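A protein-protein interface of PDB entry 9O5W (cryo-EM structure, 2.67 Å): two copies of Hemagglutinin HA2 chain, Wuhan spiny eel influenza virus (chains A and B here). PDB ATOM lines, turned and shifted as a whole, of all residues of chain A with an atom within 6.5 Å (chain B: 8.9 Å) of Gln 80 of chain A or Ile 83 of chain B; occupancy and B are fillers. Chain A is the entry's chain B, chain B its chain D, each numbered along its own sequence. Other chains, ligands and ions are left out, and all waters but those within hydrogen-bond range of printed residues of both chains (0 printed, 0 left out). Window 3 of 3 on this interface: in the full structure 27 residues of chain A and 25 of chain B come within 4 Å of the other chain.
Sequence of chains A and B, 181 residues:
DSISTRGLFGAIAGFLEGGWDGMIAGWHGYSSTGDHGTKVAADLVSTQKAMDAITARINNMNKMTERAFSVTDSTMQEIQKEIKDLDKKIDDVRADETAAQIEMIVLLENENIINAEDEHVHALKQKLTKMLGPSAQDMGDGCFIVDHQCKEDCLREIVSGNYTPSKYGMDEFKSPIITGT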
ATOM      1  N   GLU A  78      14.768 -24.980 -28.977  1.00  0.00           N
ATOM      2  CA  GLU A  78      14.090 -25.060 -27.676  1.00  0.00           C
ATOM      3  C   GLU A  78      14.766 -26.077 -26.758  1.00  0.00           C
ATOM      4  O   GLU A  78      14.111 -26.802 -26.005  1.00  0.00           O
ATOM      5  CB  GLU A  78      12.599 -25.377 -27.835  1.00  0.00           C
ATOM      6  CG  GLU A  78      11.797 -24.256 -28.473  1.00  0.00           C
ATOM      7  CD  GLU A  78      11.302 -23.235 -27.461  1.00  0.00           C
ATOM      8  OE1 GLU A  78      10.385 -22.459 -27.802  1.00  0.00           O
ATOM      9  OE2 GLU A  78      11.834 -23.198 -26.330  1.00  0.00           O
ATOM     10  N   ILE A  79      16.093 -26.133 -26.837  1.00  0.00           N
ATOM     11  CA  ILE A  79      16.933 -26.993 -26.011  1.00  0.00           C
ATOM     12  C   ILE A  79      17.912 -26.108 -25.256  1.00  0.00           C
ATOM     13  O   ILE A  79      17.768 -24.880 -25.264  1.00  0.00           O
ATOM     14  CB  ILE A  79      17.656 -28.061 -26.857  1.00  0.00           C
ATOM     15  CG1 ILE A  79      18.594 -27.415 -27.894  1.00  0.00           C
ATOM     16  CG2 ILE A  79      16.634 -28.984 -27.488  1.00  0.00           C
ATOM     17  CD1 ILE A  79      19.522 -28.371 -28.567  1.00  0.00           C
ATOM     18  N   GLN A  80      18.849 -26.735 -24.539  1.00  0.00           N
ATOM     19  CA  GLN A  80      19.879 -26.012 -23.803  1.00  0.00           C
ATOM     20  C   GLN A  80      20.519 -24.982 -24.723  1.00  0.00           C
ATOM     21  O   GLN A  80      20.872 -25.283 -25.866  1.00  0.00           O
ATOM     22  CB  GLN A  80      20.919 -26.988 -23.251  1.00  0.00           C
ATOM     23  CG  GLN A  80      22.046 -26.337 -22.466  1.00  0.00           C
ATOM     24  CD  GLN A  80      23.006 -27.353 -21.893  1.00  0.00           C
ATOM     25  OE1 GLN A  80      22.807 -28.559 -22.034  1.00  0.00           O
ATOM     26  NE2 GLN A  80      24.049 -26.872 -21.230  1.00  0.00           N
ATOM     27  N   LYS A  81      20.640 -23.757 -24.217  1.00  0.00           N
ATOM     28  CA  LYS A  81      21.151 -22.656 -25.026  1.00  0.00           C
ATOM     29  C   LYS A  81      22.561 -22.916 -25.544  1.00  0.00           C
ATOM     30  O   LYS A  81      22.869 -22.560 -26.682  1.00  0.00           O
ATOM     31  CB  LYS A  81      21.101 -21.358 -24.225  1.00  0.00           C
ATOM     32  CG  LYS A  81      21.529 -20.151 -25.021  1.00  0.00           C
ATOM     33  CD  LYS A  81      21.197 -18.865 -24.295  1.00  0.00           C
ATOM     34  CE  LYS A  81      21.836 -17.674 -24.974  1.00  0.00           C
ATOM     35  NZ  LYS A  81      21.393 -17.595 -26.392  1.00  0.00           N
ATOM     36  N   GLU A  82      23.452 -23.468 -24.716  1.00  0.00           N
ATOM     37  CA  GLU A  82      24.818 -23.709 -25.184  1.00  0.00           C
ATOM     38  C   GLU A  82      24.859 -24.658 -26.383  1.00  0.00           C
ATOM     39  O   GLU A  82      25.664 -24.463 -27.304  1.00  0.00           O
ATOM     40  CB  GLU A  82      25.681 -24.256 -24.048  1.00  0.00           C
ATOM     41  CG  GLU A  82      25.947 -23.269 -22.914  1.00  0.00           C
ATOM     42  CD  GLU A  82      24.833 -23.219 -21.888  1.00  0.00           C
ATOM     43  OE1 GLU A  82      25.097 -23.527 -20.707  1.00  0.00           O
ATOM     44  OE2 GLU A  82      23.695 -22.872 -22.263  1.00  0.00           O
ATOM     45  N   ILE A  83      23.961 -25.642 -26.430  1.00  0.00           N
ATOM     46  CA  ILE A  83      23.928 -26.573 -27.557  1.00  0.00           C
ATOM     47  C   ILE A  83      23.391 -25.860 -28.794  1.00  0.00           C
ATOM     48  O   ILE A  83      23.912 -26.025 -29.909  1.00  0.00           O
ATOM     49  CB  ILE A  83      23.109 -27.824 -27.171  1.00  0.00           C
ATOM     50  CG1 ILE A  83      23.858 -28.599 -26.070  1.00  0.00           C
ATOM     51  CG2 ILE A  83      22.863 -28.747 -28.377  1.00  0.00           C
ATOM     52  CD1 ILE A  83      23.078 -29.721 -25.400  1.00  0.00           C
ATOM     53  N   LYS A  84      22.333 -25.066 -28.612  1.00  0.00           N
ATOM     54  CA  LYS A  84      21.769 -24.286 -29.707  1.00  0.00           C
ATOM     55  C   LYS A  84      22.827 -23.358 -30.279  1.00  0.00           C
ATOM     56  O   LYS A  84      22.944 -23.193 -31.500  1.00  0.00           O
ATOM     57  CB  LYS A  84      20.600 -23.454 -29.174  1.00  0.00           C
ATOM     58  CG  LYS A  84      19.840 -22.613 -30.204  1.00  0.00           C
ATOM     59  CD  LYS A  84      18.792 -21.698 -29.550  1.00  0.00           C
ATOM     60  CE  LYS A  84      17.842 -22.393 -28.588  1.00  0.00           C
ATOM     61  NZ  LYS A  84      16.482 -21.792 -28.640  1.00  0.00           N
ATOM     62  N   ASP A  85      23.632 -22.773 -29.394  1.00  0.00           N
ATOM     63  CA  ASP A  85      24.671 -21.845 -29.799  1.00  0.00           C
ATOM     64  C   ASP A  85      25.783 -22.556 -30.550  1.00  0.00           C
ATOM     65  O   ASP A  85      26.329 -22.003 -31.506  1.00  0.00           O
ATOM     66  CB  ASP A  85      25.233 -21.133 -28.572  1.00  0.00           C
ATOM     67  CG  ASP A  85      24.262 -20.134 -27.977  1.00  0.00           C
ATOM     68  OD1 ASP A  85      23.258 -19.797 -28.638  1.00  0.00           O
ATOM     69  OD2 ASP A  85      24.507 -19.680 -26.840  1.00  0.00           O
ATOM     70  N   LEU A  86      26.154 -23.770 -30.133  1.00  0.00           N
ATOM     71  CA  LEU A  86      27.168 -24.479 -30.909  1.00  0.00           C
ATOM     72  C   LEU A  86      26.651 -24.840 -32.296  1.00  0.00           C
ATOM     73  O   LEU A  86      27.397 -24.755 -33.280  1.00  0.00           O
ATOM     74  CB  LEU A  86      27.623 -25.739 -30.178  1.00  0.00           C
ATOM     75  CG  LEU A  86      28.476 -25.589 -28.921  1.00  0.00           C
ATOM     76  CD1 LEU A  86      28.662 -26.950 -28.286  1.00  0.00           C
ATOM     77  CD2 LEU A  86      29.822 -24.957 -29.217  1.00  0.00           C
ATOM     78  N   SER B  74      28.459 -16.415 -27.560  1.00  0.00           N
ATOM     79  CA  SER B  74      29.619 -17.239 -27.288  1.00  0.00           C
ATOM     80  C   SER B  74      29.279 -18.281 -26.238  1.00  0.00           C
ATOM     81  O   SER B  74      28.311 -18.156 -25.483  1.00  0.00           O
ATOM     82  CB  SER B  74      30.790 -16.378 -26.813  1.00  0.00           C
ATOM     83  OG  SER B  74      31.930 -17.174 -26.540  1.00  0.00           O
ATOM     84  N   THR B  75      30.093 -19.326 -26.205  1.00  0.00           N
ATOM     85  CA  THR B  75      30.004 -20.339 -25.173  1.00  0.00           C
ATOM     86  C   THR B  75      30.934 -19.904 -24.052  1.00  0.00           C
ATOM     87  O   THR B  75      32.103 -19.592 -24.305  1.00  0.00           O
ATOM     88  CB  THR B  75      30.389 -21.707 -25.741  1.00  0.00           C
ATOM     89  OG1 THR B  75      29.466 -22.065 -26.777  1.00  0.00           O
ATOM     90  CG2 THR B  75      30.342 -22.780 -24.684  1.00  0.00           C
ATOM     91  N   MET B  76      30.430 -19.888 -22.823  1.00  0.00           N
ATOM     92  CA  MET B  76      31.291 -19.460 -21.735  1.00  0.00           C
ATOM     93  C   MET B  76      32.150 -20.626 -21.276  1.00  0.00           C
ATOM     94  O   MET B  76      31.844 -21.795 -21.518  1.00  0.00           O
ATOM     95  CB  MET B  76      30.503 -18.928 -20.533  1.00  0.00           C
ATOM     96  CG  MET B  76      29.191 -18.212 -20.824  1.00  0.00           C
ATOM     97  SD  MET B  76      28.305 -17.718 -19.324  1.00  0.00           S
ATOM     98  CE  MET B  76      27.959 -19.271 -18.498  1.00  0.00           C
ATOM     99  N   GLN B  77      33.250 -20.287 -20.619  1.00  0.00           N
ATOM    100  CA  GLN B  77      34.138 -21.283 -20.055  1.00  0.00           C
ATOM    101  C   GLN B  77      33.572 -21.697 -18.698  1.00  0.00           C
ATOM    102  O   GLN B  77      32.547 -21.176 -18.249  1.00  0.00           O
ATOM    103  CB  GLN B  77      35.549 -20.711 -19.949  1.00  0.00           C
ATOM    104  CG  GLN B  77      36.133 -20.236 -21.286  1.00  0.00           C
ATOM    105  CD  GLN B  77      36.376 -21.359 -22.273  1.00  0.00           C
ATOM    106  OE1 GLN B  77      35.589 -21.575 -23.193  1.00  0.00           O
ATOM    107  NE2 GLN B  77      37.485 -22.069 -22.098  1.00  0.00           N
ATOM    108  N   GLU B  78      34.220 -22.654 -18.031  1.00  0.00           N
ATOM    109  CA  GLU B  78      33.766 -23.129 -16.716  1.00  0.00           C
ATOM    110  C   GLU B  78      32.364 -23.746 -16.797  1.00  0.00           C
ATOM    111  O   GLU B  78      31.539 -23.600 -15.893  1.00  0.00           O
ATOM    112  CB  GLU B  78      33.840 -21.992 -15.670  1.00  0.00           C
ATOM    113  CG  GLU B  78      35.147 -21.868 -14.871  1.00  0.00           C
ATOM    114  CD  GLU B  78      35.478 -23.063 -13.981  1.00  0.00           C
ATOM    115  OE1 GLU B  78      35.027 -24.196 -14.238  1.00  0.00           O
ATOM    116  OE2 GLU B  78      36.208 -22.852 -12.990  1.00  0.00           O
ATOM    117  N   ILE B  79      32.098 -24.449 -17.899  1.00  0.00           N
ATOM    118  CA  ILE B  79      30.836 -25.150 -18.130  1.00  0.00           C
ATOM    119  C   ILE B  79      31.138 -26.626 -18.349  1.00  0.00           C
ATOM    120  O   ILE B  79      32.271 -27.067 -18.126  1.00  0.00           O
ATOM    121  CB  ILE B  79      30.061 -24.550 -19.322  1.00  0.00           C
ATOM    122  CG1 ILE B  79      30.858 -24.686 -20.631  1.00  0.00           C
ATOM    123  CG2 ILE B  79      29.708 -23.090 -19.029  1.00  0.00           C
ATOM    124  CD1 ILE B  79      30.077 -24.379 -21.860  1.00  0.00           C
ATOM    125  N   GLN B  80      30.104 -27.400 -18.701  1.00  0.00           N
ATOM    126  CA  GLN B  80      30.253 -28.824 -18.988  1.00  0.00           C
ATOM    127  C   GLN B  80      31.410 -29.020 -19.958  1.00  0.00           C
ATOM    128  O   GLN B  80      31.516 -28.321 -20.969  1.00  0.00           O
ATOM    129  CB  GLN B  80      28.952 -29.392 -19.561  1.00  0.00           C
ATOM    130  CG  GLN B  80      29.002 -30.877 -19.900  1.00  0.00           C
ATOM    131  CD  GLN B  80      27.676 -31.400 -20.402  1.00  0.00           C
ATOM    132  OE1 GLN B  80      26.687 -30.669 -20.452  1.00  0.00           O
ATOM    133  NE2 GLN B  80      27.643 -32.674 -20.771  1.00  0.00           N
ATOM    134  N   LYS B  81      32.284 -29.969 -19.628  1.00  0.00           N
ATOM    135  CA  LYS B  81      33.487 -30.189 -20.423  1.00  0.00           C
ATOM    136  C   LYS B  81      33.186 -30.555 -21.873  1.00  0.00           C
ATOM    137  O   LYS B  81      33.893 -30.100 -22.774  1.00  0.00           O
ATOM    138  CB  LYS B  81      34.343 -31.269 -19.764  1.00  0.00           C
ATOM    139  CG  LYS B  81      35.657 -31.503 -20.466  1.00  0.00           C
ATOM    140  CD  LYS B  81      36.581 -32.360 -19.627  1.00  0.00           C
ATOM    141  CE  LYS B  81      37.797 -32.795 -20.415  1.00  0.00           C
ATOM    142  NZ  LYS B  81      38.522 -31.599 -20.921  1.00  0.00           N
ATOM    143  N   GLU B  82      32.197 -31.418 -22.127  1.00  0.00           N
ATOM    144  CA  GLU B  82      31.914 -31.791 -23.515  1.00  0.00           C
ATOM    145  C   GLU B  82      31.515 -30.591 -24.375  1.00  0.00           C
ATOM    146  O   GLU B  82      31.912 -30.503 -25.546  1.00  0.00           O
ATOM    147  CB  GLU B  82      30.825 -32.862 -23.567  1.00  0.00           C
ATOM    148  CG  GLU B  82      31.227 -34.219 -22.995  1.00  0.00           C
ATOM    149  CD  GLU B  82      31.076 -34.308 -21.491  1.00  0.00           C
ATOM    150  OE1 GLU B  82      30.614 -35.359 -21.002  1.00  0.00           O
ATOM    151  OE2 GLU B  82      31.420 -33.329 -20.797  1.00  0.00           O
ATOM    152  N   ILE B  83      30.801 -29.623 -23.799  1.00  0.00           N
ATOM    153  CA  ILE B  83      30.400 -28.436 -24.551  1.00  0.00           C
ATOM    154  C   ILE B  83      31.616 -27.550 -24.797  1.00  0.00           C
ATOM    155  O   ILE B  83      31.812 -27.012 -25.899  1.00  0.00           O
ATOM    156  CB  ILE B  83      29.264 -27.711 -23.800  1.00  0.00           C
ATOM    157  CG1 ILE B  83      28.003 -28.598 -23.809  1.00  0.00           C
ATOM    158  CG2 ILE B  83      28.950 -26.335 -24.413  1.00  0.00           C
ATOM    159  CD1 ILE B  83      26.869 -28.146 -22.902  1.00  0.00           C
ATOM    160  N   LYS B  84      32.444 -27.381 -23.764  1.00  0.00           N
ATOM    161  CA  LYS B  84      33.671 -26.607 -23.887  1.00  0.00           C
ATOM    162  C   LYS B  84      34.556 -27.207 -24.967  1.00  0.00           C
ATOM    163  O   LYS B  84      35.157 -26.489 -25.777  1.00  0.00           O
ATOM    164  CB  LYS B  84      34.401 -26.631 -22.543  1.00  0.00           C
ATOM    165  CG  LYS B  84      35.684 -25.823 -22.443  1.00  0.00           C
ATOM    166  CD  LYS B  84      36.356 -26.075 -21.094  1.00  0.00           C
ATOM    167  CE  LYS B  84      35.637 -25.417 -19.930  1.00  0.00           C
ATOM    168  NZ  LYS B  84      36.586 -25.058 -18.839  1.00  0.00           N
ATOM    169  N   ASP B  85      34.604 -28.537 -25.010  1.00  0.00           N
ATOM    170  CA  ASP B  85      35.426 -29.243 -25.975  1.00  0.00           C
ATOM    171  C   ASP B  85      34.884 -29.078 -27.384  1.00  0.00           C
ATOM    172  O   ASP B  85      35.664 -28.959 -28.328  1.00  0.00           O
ATOM    173  CB  ASP B  85      35.500 -30.724 -25.607  1.00  0.00           C
ATOM    174  CG  ASP B  85      36.340 -30.981 -24.373  1.00  0.00           C
ATOM    175  OD1 ASP B  85      37.074 -30.069 -23.937  1.00  0.00           O
ATOM    176  OD2 ASP B  85      36.269 -32.106 -23.836  1.00  0.00           O
ATOM    177  N   LEU B  86      33.560 -29.090 -27.562  1.00  0.00           N
ATOM    178  CA  LEU B  86      33.052 -28.850 -28.911  1.00  0.00           C
ATOM    179  C   LEU B  86      33.350 -27.430 -29.376  1.00  0.00           C
ATOM    180  O   LEU B  86      33.694 -27.218 -30.546  1.00  0.00           O
ATOM    181  CB  LEU B  86      31.550 -29.110 -28.978  1.00  0.00           C
ATOM    182  CG  LEU B  86      31.044 -30.546 -28.890  1.00  0.00           C
ATOM    183  CD1 LEU B  86      29.533 -30.532 -28.812  1.00  0.00           C
ATOM    184  CD2 LEU B  86      31.500 -31.377 -30.068  1.00  0.00           C
ATOM    185  N   ASP B  87      33.253 -26.444 -28.478  1.00  0.00           N
ATOM    186  CA  ASP B  87      33.546 -25.072 -28.893  1.00  0.00           C
ATOM    187  C   ASP B  87      35.015 -24.941 -29.277  1.00  0.00           C
ATOM    188  O   ASP B  87      35.369 -24.341 -30.310  1.00  0.00           O
ATOM    189  CB  ASP B  87      33.199 -24.095 -27.770  1.00  0.00           C
ATOM    190  CG  ASP B  87      33.217 -22.650 -28.228  1.00  0.00           C
ATOM    191  OD1 ASP B  87      32.341 -22.268 -29.031  1.00  0.00           O
ATOM    192  OD2 ASP B  87      34.104 -21.894 -27.780  1.00  0.00           O
ATOM    193  N   LYS B  88      35.875 -25.581 -28.487  1.00  0.00           N
ATOM    194  CA  LYS B  88      37.302 -25.569 -28.748  1.00  0.00           C
ATOM    195  C   LYS B  88      37.600 -26.278 -30.062  1.00  0.00           C
ATOM    196  O   LYS B  88      38.463 -25.841 -30.829  1.00  0.00           O
ATOM    197  CB  LYS B  88      38.012 -26.213 -27.561  1.00  0.00           C
ATOM    198  CG  LYS B  88      39.536 -26.229 -27.613  1.00  0.00           C
ATOM    199  CD  LYS B  88      40.236 -26.569 -26.256  1.00  0.00           C
ATOM    200  CE  LYS B  88      39.766 -25.788 -25.000  1.00  0.00           C
ATOM    201  NZ  LYS B  88      40.234 -26.421 -23.735  1.00  0.00           N
ATOM    202  N   LYS B  89      36.927 -27.406 -30.312  1.00  0.00           N
ATOM    203  CA  LYS B  89      37.130 -28.146 -31.550  1.00  0.00           C
ATOM    204  C   LYS B  89      36.753 -27.297 -32.753  1.00  0.00           C
ATOM    205  O   LYS B  89      37.433 -27.339 -33.783  1.00  0.00           O
ATOM    206  CB  LYS B  89      36.301 -29.431 -31.536  1.00  0.00           C
ATOM    207  CG  LYS B  89      36.521 -30.330 -32.744  1.00  0.00           C
ATOM    208  CD  LYS B  89      35.719 -31.608 -32.637  1.00  0.00           C
ATOM    209  CE  LYS B  89      35.965 -32.505 -33.834  1.00  0.00           C
ATOM    210  NZ  LYS B  89      35.137 -33.735 -33.787  1.00  0.00           N
ATOM    211  N   ILE B  90      35.652 -26.549 -32.658  1.00  0.00           N
ATOM    212  CA  ILE B  90      35.234 -25.723 -33.789  1.00  0.00           C
ATOM    213  C   ILE B  90      36.312 -24.689 -34.077  1.00  0.00           C
ATOM    214  O   ILE B  90      36.728 -24.493 -35.231  1.00  0.00           O
ATOM    215  CB  ILE B  90      33.862 -25.072 -33.510  1.00  0.00           C
ATOM    216  CG1 ILE B  90      32.769 -26.146 -33.440  1.00  0.00           C
ATOM    217  CG2 ILE B  90      33.493 -24.027 -34.597  1.00  0.00           C
ATOM    218  CD1 ILE B  90      31.435 -25.679 -32.866  1.00  0.00           C
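Among the printed residues, pairs that only touch across the chains: Gln 80 of chain A with Ile 83 of chain B (3.5 Å), Glu 82 of chain A with Ile 83 of chain B (3.9 Å), Leu 86 of chain A with Thr 75 of chain B (3.8 Å), Leu 86 of chain A with Ile 83 of chain B (3.9 Å), Leu 86 of chain A with Leu 86 of chain B (3.7 Å) and Leu 86 of chain A with Asp 87 of chain B (3.7 Å).
Gln 80 of chain A touches Ile 83 of chain B, but with the chains exchanged Ile 83 of chain A does not touch Gln 80 of chain B (6.2 Å).
Glu 82 of chain A touches Ile 83 of chain B, but with the chains exchanged Ile 83 of chain A does not touch Glu 82 of chain B (8.1 Å).
Leu 86 of chain A touches Ile 83 of chain B, but with the chains exchanged Ile 83 of chain A does not touch Leu 86 of chain B (6.6 Å).
Leu 86 of chain A touches its own counterpart, Leu 86 of chain B.
Positions printed for both chains: 78, 79, 80, 81, 82, 83, 84, 85 and 86.
Of the 17 printed residues of chain B, 4 touch a printed residue of chain A.
Printed residues of chain B that touch a printed residue of chain A: Thr 75, Ile 83, Leu 86 and Asp 87.
Along chain B the printed residues that touch a printed residue of chain A span positions 75 to 87.
Of the 9 printed residues of chain A, 3 touch a printed residue of chain B.
Along chain A the printed residues that touch a printed residue of chain B span positions 80 to 86.
Among the printed residues, 6 pairs touch across the chains.
Among the printed residues, no Asp or Glu carboxylate lies within 4 Å of a Lys or Arg side-chain nitrogen of the other chain.
Gln 80 of chain A touches just one residue of chain B: Ile 83.
Of chain B, only Ile 83 comes within 4 Å of Glu 82 of chain A.
Of the printed residues of chain B, Leu 86 of chain A touches Thr 75 (3.8 Å), Ile 83 (3.9 Å), Leu 86 (3.7 Å) and Asp 87 (3.7 Å).
Printed residues of chain A within 4 Å of Thr 75 of chain B: Leu 86.
Gln 80 of chain B touches none of the printed residues of chain A.
Of the printed residues of chain A, Ile 83 of chain B touches Gln 80, Glu 82 and Leu 86.
Printed residues of chain A within 4 Å of Leu 86 of chain B: Leu 86 (3.7 Å).
The nearest residue of chain A that does not touch Ile 83 of chain B is Ile 83 of chain A (4.4 Å).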
